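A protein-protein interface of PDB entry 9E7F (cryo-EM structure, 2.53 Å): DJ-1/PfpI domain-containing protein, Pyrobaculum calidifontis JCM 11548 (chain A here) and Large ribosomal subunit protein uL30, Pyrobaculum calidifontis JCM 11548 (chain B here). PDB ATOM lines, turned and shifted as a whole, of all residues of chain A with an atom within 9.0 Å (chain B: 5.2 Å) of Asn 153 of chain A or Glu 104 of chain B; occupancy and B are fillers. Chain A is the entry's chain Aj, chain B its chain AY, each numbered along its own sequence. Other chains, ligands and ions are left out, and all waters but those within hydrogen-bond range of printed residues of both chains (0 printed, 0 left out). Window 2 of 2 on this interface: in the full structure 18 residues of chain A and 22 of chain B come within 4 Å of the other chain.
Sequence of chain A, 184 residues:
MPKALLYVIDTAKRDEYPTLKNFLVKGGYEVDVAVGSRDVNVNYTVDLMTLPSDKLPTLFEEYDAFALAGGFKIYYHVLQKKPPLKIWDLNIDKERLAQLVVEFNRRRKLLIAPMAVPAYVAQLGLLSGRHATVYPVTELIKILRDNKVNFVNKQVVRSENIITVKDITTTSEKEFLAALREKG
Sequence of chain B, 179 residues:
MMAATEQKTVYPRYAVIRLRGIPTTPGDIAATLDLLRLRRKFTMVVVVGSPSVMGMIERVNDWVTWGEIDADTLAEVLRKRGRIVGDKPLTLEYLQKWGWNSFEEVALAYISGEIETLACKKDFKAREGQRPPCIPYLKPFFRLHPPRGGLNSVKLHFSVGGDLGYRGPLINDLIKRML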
ATOM      1  N   HIS A 131      -4.346 -26.248   3.574  1.00  0.00           N
ATOM      2  CA  HIS A 131      -4.131 -26.023   2.152  1.00  0.00           C
ATOM      3  C   HIS A 131      -4.367 -27.329   1.407  1.00  0.00           C
ATOM      4  O   HIS A 131      -3.672 -28.318   1.651  1.00  0.00           O
ATOM      5  CB  HIS A 131      -2.719 -25.508   1.883  1.00  0.00           C
ATOM      6  CG  HIS A 131      -2.436 -24.174   2.495  1.00  0.00           C
ATOM      7  ND1 HIS A 131      -3.215 -23.065   2.250  1.00  0.00           N
ATOM      8  CD2 HIS A 131      -1.459 -23.769   3.339  1.00  0.00           C
ATOM      9  CE1 HIS A 131      -2.731 -22.034   2.919  1.00  0.00           C
ATOM     10  NE2 HIS A 131      -1.666 -22.436   3.588  1.00  0.00           N
ATOM     11  N   ALA A 132      -5.331 -27.323   0.493  1.00  0.00           N
ATOM     12  CA  ALA A 132      -5.699 -28.537  -0.217  1.00  0.00           C
ATOM     13  C   ALA A 132      -6.085 -28.192  -1.644  1.00  0.00           C
ATOM     14  O   ALA A 132      -6.385 -27.043  -1.971  1.00  0.00           O
ATOM     15  CB  ALA A 132      -6.846 -29.274   0.481  1.00  0.00           C
ATOM     16  N   THR A 133      -6.070 -29.212  -2.494  1.00  0.00           N
ATOM     17  CA  THR A 133      -6.470 -29.082  -3.883  1.00  0.00           C
ATOM     18  C   THR A 133      -7.484 -30.163  -4.217  1.00  0.00           C
ATOM     19  O   THR A 133      -7.464 -31.256  -3.650  1.00  0.00           O
ATOM     20  CB  THR A 133      -5.274 -29.182  -4.830  1.00  0.00           C
ATOM     21  OG1 THR A 133      -5.649 -28.695  -6.122  1.00  0.00           O
ATOM     22  CG2 THR A 133      -4.812 -30.617  -4.955  1.00  0.00           C
ATOM     23  N   VAL A 134      -8.382 -29.837  -5.140  1.00  0.00           N
ATOM     24  CA  VAL A 134      -9.419 -30.750  -5.595  1.00  0.00           C
ATOM     25  C   VAL A 134      -9.474 -30.633  -7.111  1.00  0.00           C
ATOM     26  O   VAL A 134      -8.810 -29.785  -7.710  1.00  0.00           O
ATOM     27  CB  VAL A 134     -10.790 -30.430  -4.948  1.00  0.00           C
ATOM     28  CG1 VAL A 134     -11.423 -29.220  -5.601  1.00  0.00           C
ATOM     29  CG2 VAL A 134     -11.726 -31.627  -4.985  1.00  0.00           C
ATOM     30  N   TYR A 135     -10.249 -31.512  -7.734  1.00  0.00           N
ATOM     31  CA  TYR A 135     -10.521 -31.418  -9.156  1.00  0.00           C
ATOM     32  C   TYR A 135     -11.207 -30.087  -9.452  1.00  0.00           C
ATOM     33  O   TYR A 135     -12.289 -29.821  -8.909  1.00  0.00           O
ATOM     34  CB  TYR A 135     -11.401 -32.579  -9.596  1.00  0.00           C
ATOM     35  CG  TYR A 135     -11.345 -32.882 -11.069  1.00  0.00           C
ATOM     36  CD1 TYR A 135     -10.229 -33.472 -11.633  1.00  0.00           C
ATOM     37  CD2 TYR A 135     -12.421 -32.599 -11.891  1.00  0.00           C
ATOM     38  CE1 TYR A 135     -10.183 -33.759 -12.972  1.00  0.00           C
ATOM     39  CE2 TYR A 135     -12.386 -32.883 -13.230  1.00  0.00           C
ATOM     40  CZ  TYR A 135     -11.265 -33.462 -13.768  1.00  0.00           C
ATOM     41  OH  TYR A 135     -11.228 -33.745 -15.110  1.00  0.00           O
ATOM     42  N   PRO A 136     -10.632 -29.247 -10.295  1.00  0.00           N
ATOM     43  CA  PRO A 136     -11.029 -27.829 -10.326  1.00  0.00           C
ATOM     44  C   PRO A 136     -12.258 -27.560 -11.184  1.00  0.00           C
ATOM     45  O   PRO A 136     -12.230 -26.853 -12.190  1.00  0.00           O
ATOM     46  CB  PRO A 136      -9.765 -27.149 -10.862  1.00  0.00           C
ATOM     47  CG  PRO A 136      -8.933 -28.239 -11.485  1.00  0.00           C
ATOM     48  CD  PRO A 136      -9.594 -29.551 -11.286  1.00  0.00           C
ATOM     49  N   VAL A 137     -13.380 -28.131 -10.769  1.00  0.00           N
ATOM     50  CA  VAL A 137     -14.678 -27.776 -11.315  1.00  0.00           C
ATOM     51  C   VAL A 137     -15.328 -26.796 -10.351  1.00  0.00           C
ATOM     52  O   VAL A 137     -14.883 -26.616  -9.215  1.00  0.00           O
ATOM     53  CB  VAL A 137     -15.582 -29.004 -11.551  1.00  0.00           C
ATOM     54  CG1 VAL A 137     -15.050 -29.834 -12.704  1.00  0.00           C
ATOM     55  CG2 VAL A 137     -15.695 -29.835 -10.288  1.00  0.00           C
ATOM     56  N   ILE A 141     -14.922 -27.018  -6.101  1.00  0.00           N
ATOM     57  CA  ILE A 141     -14.198 -25.908  -5.488  1.00  0.00           C
ATOM     58  C   ILE A 141     -15.066 -25.229  -4.440  1.00  0.00           C
ATOM     59  O   ILE A 141     -14.578 -24.794  -3.392  1.00  0.00           O
ATOM     60  CB  ILE A 141     -13.732 -24.909  -6.561  1.00  0.00           C
ATOM     61  CG1 ILE A 141     -12.653 -25.524  -7.447  1.00  0.00           C
ATOM     62  CG2 ILE A 141     -13.202 -23.649  -5.916  1.00  0.00           C
ATOM     63  CD1 ILE A 141     -12.301 -24.674  -8.637  1.00  0.00           C
ATOM     64  N   ARG A 145     -14.756 -24.818  -0.077  1.00  0.00           N
ATOM     65  CA  ARG A 145     -14.844 -23.493   0.524  1.00  0.00           C
ATOM     66  C   ARG A 145     -15.800 -23.472   1.708  1.00  0.00           C
ATOM     67  O   ARG A 145     -15.493 -22.879   2.747  1.00  0.00           O
ATOM     68  CB  ARG A 145     -15.262 -22.468  -0.524  1.00  0.00           C
ATOM     69  CG  ARG A 145     -14.138 -21.558  -0.955  1.00  0.00           C
ATOM     70  CD  ARG A 145     -13.464 -22.091  -2.194  1.00  0.00           C
ATOM     71  NE  ARG A 145     -12.313 -21.284  -2.578  1.00  0.00           N
ATOM     72  CZ  ARG A 145     -12.272 -20.492  -3.641  1.00  0.00           C
ATOM     73  NH1 ARG A 145     -13.308 -20.370  -4.452  1.00  0.00           N
ATOM     74  NH2 ARG A 145     -11.164 -19.805  -3.894  1.00  0.00           N
ATOM     75  N   ASN A 150      -8.652 -24.211   2.322  1.00  0.00           N
ATOM     76  CA  ASN A 150      -7.997 -23.221   1.477  1.00  0.00           C
ATOM     77  C   ASN A 150      -7.609 -23.882   0.161  1.00  0.00           C
ATOM     78  O   ASN A 150      -6.644 -24.645   0.095  1.00  0.00           O
ATOM     79  CB  ASN A 150      -6.783 -22.639   2.189  1.00  0.00           C
ATOM     80  CG  ASN A 150      -7.093 -22.223   3.612  1.00  0.00           C
ATOM     81  OD1 ASN A 150      -8.236 -22.300   4.058  1.00  0.00           O
ATOM     82  ND2 ASN A 150      -6.071 -21.785   4.336  1.00  0.00           N
ATOM     83  N   PHE A 151      -8.363 -23.587  -0.894  1.00  0.00           N
ATOM     84  CA  PHE A 151      -8.067 -24.140  -2.207  1.00  0.00           C
ATOM     85  C   PHE A 151      -6.757 -23.580  -2.736  1.00  0.00           C
ATOM     86  O   PHE A 151      -6.488 -22.381  -2.633  1.00  0.00           O
ATOM     87  CB  PHE A 151      -9.200 -23.828  -3.184  1.00  0.00           C
ATOM     88  CG  PHE A 151      -8.906 -24.217  -4.608  1.00  0.00           C
ATOM     89  CD1 PHE A 151      -8.752 -25.543  -4.962  1.00  0.00           C
ATOM     90  CD2 PHE A 151      -8.788 -23.253  -5.589  1.00  0.00           C
ATOM     91  CE1 PHE A 151      -8.486 -25.900  -6.265  1.00  0.00           C
ATOM     92  CE2 PHE A 151      -8.519 -23.606  -6.897  1.00  0.00           C
ATOM     93  CZ  PHE A 151      -8.367 -24.931  -7.234  1.00  0.00           C
ATOM     94  N   VAL A 152      -5.943 -24.459  -3.306  1.00  0.00           N
ATOM     95  CA  VAL A 152      -4.682 -24.090  -3.934  1.00  0.00           C
ATOM     96  C   VAL A 152      -4.697 -24.618  -5.360  1.00  0.00           C
ATOM     97  O   VAL A 152      -5.114 -25.754  -5.605  1.00  0.00           O
ATOM     98  CB  VAL A 152      -3.472 -24.645  -3.158  1.00  0.00           C
ATOM     99  CG1 VAL A 152      -2.193 -24.334  -3.889  1.00  0.00           C
ATOM    100  CG2 VAL A 152      -3.434 -24.070  -1.760  1.00  0.00           C
ATOM    101  N   ASN A 153      -4.231 -23.802  -6.299  1.00  0.00           N
ATOM    102  CA  ASN A 153      -4.237 -24.160  -7.709  1.00  0.00           C
ATOM    103  C   ASN A 153      -2.999 -24.947  -8.122  1.00  0.00           C
ATOM    104  O   ASN A 153      -2.601 -24.889  -9.290  1.00  0.00           O
ATOM    105  CB  ASN A 153      -4.369 -22.905  -8.571  1.00  0.00           C
ATOM    106  CG  ASN A 153      -5.133 -23.159  -9.852  1.00  0.00           C
ATOM    107  OD1 ASN A 153      -5.755 -24.207 -10.019  1.00  0.00           O
ATOM    108  ND2 ASN A 153      -5.103 -22.194 -10.761  1.00  0.00           N
ATOM    109  N   LYS A 154      -2.376 -25.661  -7.191  1.00  0.00           N
ATOM    110  CA  LYS A 154      -1.260 -26.542  -7.488  1.00  0.00           C
ATOM    111  C   LYS A 154      -1.778 -27.954  -7.749  1.00  0.00           C
ATOM    112  O   LYS A 154      -2.831 -28.349  -7.242  1.00  0.00           O
ATOM    113  CB  LYS A 154      -0.254 -26.532  -6.333  1.00  0.00           C
ATOM    114  CG  LYS A 154       0.909 -27.491  -6.486  1.00  0.00           C
ATOM    115  CD  LYS A 154       2.089 -27.111  -5.626  1.00  0.00           C
ATOM    116  CE  LYS A 154       3.313 -27.872  -6.087  1.00  0.00           C
ATOM    117  NZ  LYS A 154       2.973 -28.779  -7.218  1.00  0.00           N
ATOM    118  N   GLN A 155      -1.043 -28.696  -8.580  1.00  0.00           N
ATOM    119  CA  GLN A 155      -1.435 -30.062  -8.911  1.00  0.00           C
ATOM    120  C   GLN A 155      -1.421 -30.955  -7.680  1.00  0.00           C
ATOM    121  O   GLN A 155      -2.381 -31.691  -7.423  1.00  0.00           O
ATOM    122  CB  GLN A 155      -0.508 -30.623  -9.985  1.00  0.00           C
ATOM    123  CG  GLN A 155      -0.998 -31.912 -10.601  1.00  0.00           C
ATOM    124  CD  GLN A 155      -1.879 -31.675 -11.806  1.00  0.00           C
ATOM    125  OE1 GLN A 155      -1.797 -30.634 -12.453  1.00  0.00           O
ATOM    126  NE2 GLN A 155      -2.734 -32.641 -12.113  1.00  0.00           N
ATOM    127  N   VAL A 156      -0.346 -30.903  -6.900  1.00  0.00           N
ATOM    128  CA  VAL A 156      -0.193 -31.726  -5.707  1.00  0.00           C
ATOM    129  C   VAL A 156      -0.026 -30.807  -4.510  1.00  0.00           C
ATOM    130  O   VAL A 156       0.894 -29.984  -4.477  1.00  0.00           O
ATOM    131  CB  VAL A 156       1.002 -32.688  -5.821  1.00  0.00           C
ATOM    132  CG1 VAL A 156       1.108 -33.517  -4.567  1.00  0.00           C
ATOM    133  CG2 VAL A 156       0.852 -33.578  -7.031  1.00  0.00           C
ATOM    134  N   VAL A 157      -0.914 -30.945  -3.532  1.00  0.00           N
ATOM    135  CA  VAL A 157      -0.888 -30.134  -2.323  1.00  0.00           C
ATOM    136  C   VAL A 157      -0.942 -31.070  -1.130  1.00  0.00           C
ATOM    137  O   VAL A 157      -1.861 -31.889  -1.021  1.00  0.00           O
ATOM    138  CB  VAL A 157      -2.050 -29.131  -2.274  1.00  0.00           C
ATOM    139  CG1 VAL A 157      -1.949 -28.269  -1.029  1.00  0.00           C
ATOM    140  CG2 VAL A 157      -2.056 -28.271  -3.528  1.00  0.00           C
ATOM    141  N   LYS A 166      -4.873 -32.831  -7.960  1.00  0.00           N
ATOM    142  CA  LYS A 166      -5.972 -32.409  -8.821  1.00  0.00           C
ATOM    143  C   LYS A 166      -6.473 -33.565  -9.673  1.00  0.00           C
ATOM    144  O   LYS A 166      -7.683 -33.749  -9.839  1.00  0.00           O
ATOM    145  CB  LYS A 166      -5.533 -31.241  -9.702  1.00  0.00           C
ATOM    146  CG  LYS A 166      -5.548 -29.903  -9.004  1.00  0.00           C
ATOM    147  CD  LYS A 166      -5.971 -28.809  -9.949  1.00  0.00           C
ATOM    148  CE  LYS A 166      -4.780 -28.253 -10.708  1.00  0.00           C
ATOM    149  NZ  LYS A 166      -4.808 -26.771 -10.800  1.00  0.00           N
ATOM    150  N   GLU A 175       6.299 -34.307  -9.714  1.00  0.00           N
ATOM    151  CA  GLU A 175       5.492 -33.539  -8.772  1.00  0.00           C
ATOM    152  C   GLU A 175       4.924 -34.432  -7.676  1.00  0.00           C
ATOM    153  O   GLU A 175       4.893 -34.044  -6.504  1.00  0.00           O
ATOM    154  CB  GLU A 175       4.365 -32.825  -9.511  1.00  0.00           C
ATOM    155  CG  GLU A 175       4.786 -32.213 -10.828  1.00  0.00           C
ATOM    156  CD  GLU A 175       3.606 -31.731 -11.644  1.00  0.00           C
ATOM    157  OE1 GLU A 175       2.477 -31.742 -11.115  1.00  0.00           O
ATOM    158  OE2 GLU A 175       3.807 -31.347 -12.813  1.00  0.00           O
ATOM    159  N   ALA B  71     -10.809 -26.211 -14.377  1.00  0.00           N
ATOM    160  CA  ALA B  71      -9.996 -25.018 -14.578  1.00  0.00           C
ATOM    161  C   ALA B  71      -8.733 -25.328 -15.369  1.00  0.00           C
ATOM    162  O   ALA B  71      -8.278 -24.506 -16.169  1.00  0.00           O
ATOM    163  CB  ALA B  71      -9.643 -24.390 -13.234  1.00  0.00           C
ATOM    164  N   ASP B  72      -8.147 -26.505 -15.155  1.00  0.00           N
ATOM    165  CA  ASP B  72      -6.908 -26.835 -15.849  1.00  0.00           C
ATOM    166  C   ASP B  72      -7.150 -27.103 -17.327  1.00  0.00           C
ATOM    167  O   ASP B  72      -6.342 -26.708 -18.173  1.00  0.00           O
ATOM    168  CB  ASP B  72      -6.237 -28.033 -15.186  1.00  0.00           C
ATOM    169  CG  ASP B  72      -4.975 -27.648 -14.443  1.00  0.00           C
ATOM    170  OD1 ASP B  72      -4.705 -26.434 -14.319  1.00  0.00           O
ATOM    171  OD2 ASP B  72      -4.248 -28.554 -13.982  1.00  0.00           O
ATOM    172  N   ALA B  75      -7.685 -23.865 -19.145  1.00  0.00           N
ATOM    173  CA  ALA B  75      -6.440 -23.126 -19.319  1.00  0.00           C
ATOM    174  C   ALA B  75      -5.701 -23.574 -20.575  1.00  0.00           C
ATOM    175  O   ALA B  75      -5.198 -22.747 -21.341  1.00  0.00           O
ATOM    176  CB  ALA B  75      -5.560 -23.291 -18.082  1.00  0.00           C
ATOM    177  N   ARG B  79      -5.111 -21.557 -24.264  1.00  0.00           N
ATOM    178  CA  ARG B  79      -3.799 -21.375 -24.869  1.00  0.00           C
ATOM    179  C   ARG B  79      -3.728 -22.013 -26.251  1.00  0.00           C
ATOM    180  O   ARG B  79      -3.159 -21.429 -27.180  1.00  0.00           O
ATOM    181  CB  ARG B  79      -2.724 -21.955 -23.954  1.00  0.00           C
ATOM    182  CG  ARG B  79      -1.335 -21.415 -24.203  1.00  0.00           C
ATOM    183  CD  ARG B  79      -0.284 -22.231 -23.473  1.00  0.00           C
ATOM    184  NE  ARG B  79      -0.873 -23.202 -22.561  1.00  0.00           N
ATOM    185  CZ  ARG B  79      -1.039 -23.004 -21.260  1.00  0.00           C
ATOM    186  NH1 ARG B  79      -0.658 -21.879 -20.678  1.00  0.00           N
ATOM    187  NH2 ARG B  79      -1.602 -23.958 -20.525  1.00  0.00           N
ATOM    188  N   SER B 102      -1.453 -15.174 -15.931  1.00  0.00           N
ATOM    189  CA  SER B 102      -1.276 -16.495 -16.513  1.00  0.00           C
ATOM    190  C   SER B 102      -2.606 -17.003 -17.042  1.00  0.00           C
ATOM    191  O   SER B 102      -3.674 -16.510 -16.674  1.00  0.00           O
ATOM    192  CB  SER B 102      -0.705 -17.484 -15.496  1.00  0.00           C
ATOM    193  OG  SER B 102      -1.670 -17.801 -14.511  1.00  0.00           O
ATOM    194  N   PHE B 103      -2.522 -17.998 -17.928  1.00  0.00           N
ATOM    195  CA  PHE B 103      -3.726 -18.646 -18.430  1.00  0.00           C
ATOM    196  C   PHE B 103      -4.486 -19.333 -17.305  1.00  0.00           C
ATOM    197  O   PHE B 103      -5.720 -19.310 -17.275  1.00  0.00           O
ATOM    198  CB  PHE B 103      -3.370 -19.657 -19.517  1.00  0.00           C
ATOM    199  CG  PHE B 103      -3.027 -19.041 -20.840  1.00  0.00           C
ATOM    200  CD1 PHE B 103      -4.020 -18.673 -21.725  1.00  0.00           C
ATOM    201  CD2 PHE B 103      -1.709 -18.855 -21.211  1.00  0.00           C
ATOM    202  CE1 PHE B 103      -3.704 -18.119 -22.944  1.00  0.00           C
ATOM    203  CE2 PHE B 103      -1.390 -18.303 -22.430  1.00  0.00           C
ATOM    204  CZ  PHE B 103      -2.388 -17.934 -23.296  1.00  0.00           C
ATOM    205  N   GLU B 104      -3.762 -19.956 -16.375  1.00  0.00           N
ATOM    206  CA  GLU B 104      -4.407 -20.681 -15.286  1.00  0.00           C
ATOM    207  C   GLU B 104      -5.150 -19.736 -14.354  1.00  0.00           C
ATOM    208  O   GLU B 104      -6.198 -20.091 -13.803  1.00  0.00           O
ATOM    209  CB  GLU B 104      -3.368 -21.481 -14.509  1.00  0.00           C
ATOM    210  CG  GLU B 104      -2.674 -22.542 -15.328  1.00  0.00           C
ATOM    211  CD  GLU B 104      -1.374 -22.053 -15.925  1.00  0.00           C
ATOM    212  OE1 GLU B 104      -1.273 -22.003 -17.169  1.00  0.00           O
ATOM    213  OE2 GLU B 104      -0.454 -21.714 -15.153  1.00  0.00           O
ATOM    214  N   GLU B 105      -4.612 -18.534 -14.149  1.00  0.00           N
ATOM    215  CA  GLU B 105      -5.258 -17.581 -13.256  1.00  0.00           C
ATOM    216  C   GLU B 105      -6.584 -17.096 -13.827  1.00  0.00           C
ATOM    217  O   GLU B 105      -7.572 -16.969 -13.098  1.00  0.00           O
ATOM    218  CB  GLU B 105      -4.321 -16.408 -12.987  1.00  0.00           C
ATOM    219  CG  GLU B 105      -4.749 -15.522 -11.841  1.00  0.00           C
ATOM    220  CD  GLU B 105      -4.883 -14.072 -12.250  1.00  0.00           C
ATOM    221  OE1 GLU B 105      -4.356 -13.702 -13.319  1.00  0.00           O
ATOM    222  OE2 GLU B 105      -5.518 -13.300 -11.501  1.00  0.00           O
ATOM    223  N   VAL B 106      -6.624 -16.809 -15.128  1.00  0.00           N
ATOM    224  CA  VAL B 106      -7.871 -16.360 -15.737  1.00  0.00           C
ATOM    225  C   VAL B 106      -8.862 -17.513 -15.836  1.00  0.00           C
ATOM    226  O   VAL B 106     -10.076 -17.312 -15.726  1.00  0.00           O
ATOM    227  CB  VAL B 106      -7.598 -15.700 -17.105  1.00  0.00           C
ATOM    228  CG1 VAL B 106      -7.191 -16.722 -18.147  1.00  0.00           C
ATOM    229  CG2 VAL B 106      -8.814 -14.922 -17.573  1.00  0.00           C
ATOM    230  N   ALA B 107      -8.370 -18.736 -16.035  1.00  0.00           N
ATOM    231  CA  ALA B 107      -9.262 -19.887 -16.112  1.00  0.00           C
ATOM    232  C   ALA B 107      -9.840 -20.229 -14.747  1.00  0.00           C
ATOM    233  O   ALA B 107     -11.002 -20.631 -14.642  1.00  0.00           O
ATOM    234  CB  ALA B 107      -8.522 -21.089 -16.694  1.00  0.00           C
ATOM    235  N   LEU B 108      -9.035 -20.088 -13.695  1.00  0.00           N
ATOM    236  CA  LEU B 108      -9.515 -20.359 -12.347  1.00  0.00           C
ATOM    237  C   LEU B 108     -10.597 -19.376 -11.934  1.00  0.00           C
ATOM    238  O   LEU B 108     -11.574 -19.760 -11.282  1.00  0.00           O
ATOM    239  CB  LEU B 108      -8.353 -20.307 -11.364  1.00  0.00           C
ATOM    240  CG  LEU B 108      -8.725 -20.597  -9.915  1.00  0.00           C
ATOM    241  CD1 LEU B 108      -9.448 -21.933  -9.794  1.00  0.00           C
ATOM    242  CD2 LEU B 108      -7.487 -20.568  -9.046  1.00  0.00           C
ATOM    243  N   ALA B 109     -10.434 -18.102 -12.293  1.00  0.00           N
ATOM    244  CA  ALA B 109     -11.393 -17.079 -11.889  1.00  0.00           C
ATOM    245  C   ALA B 109     -12.761 -17.326 -12.505  1.00  0.00           C
ATOM    246  O   ALA B 109     -13.791 -17.143 -11.848  1.00  0.00           O
ATOM    247  CB  ALA B 109     -10.877 -15.699 -12.280  1.00  0.00           C
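The backbone carbonyl oxygen (O) of Pro 136 of chain A sits at hydrogen-bond distance from the backbone NH (N) of Ala 71 of chain B, 2.7 Å away. OD1 of Asp 72 of chain B is in salt-bridge range of NZ of Lys 166 of chain A, at 3.5 Å.
The side-chain carboxylate (OE1) of Glu 104 of chain B lies within salt-bridge range of the guanidinium group (NH1) of Arg 79 of chain B. NZ of Lys 166 of chain A sits at hydrogen-bond distance from OD1 of Asn 153 of chain A. N of Lys 166 of chain A sits at hydrogen-bond distance from O of Gln 155 of chain A (2.8 Å).
Among the printed residues, merely in contact across the chains: Phe 151 of chain A with Leu 108 of chain B, Asn 153 of chain A with Glu 104 of chain B, Asn 153 of chain A with Leu 108 of chain B and Gln 155 of chain A with Asp 72 of chain B.
Asn 153 of chain A touches two residues of chain B. Of chain A, only Asn 153 (3.9 Å) comes within 4 Å of Glu 104 of chain B. No residue of chain A comes within 4 Å of Ala 107 of chain B. Printed residues of chain B within 4 Å of Phe 151 of chain A: Leu 108 (3.5 Å). Of the printed residues of chain A, Leu 108 of chain B touches Phe 151 and Asn 153. Printed residues of chain B within 4 Å of Gln 155 of chain A: Asp 72. Glu 105 of chain B touches none of the printed residues of chain A. Val 134 of chain A touches none of the printed residues of chain B.
Hydrophobic or aromatic side chains of chain A within 4 Å of the printed part of chain B: Pro 136 and Phe 151. Along chain A the printed residues that touch a printed residue of chain B span positions 136 to 166. Of the 12 printed residues of chain B, 4 touch a printed residue of chain A. Among the printed residues, 6 pairs touch across the chains.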
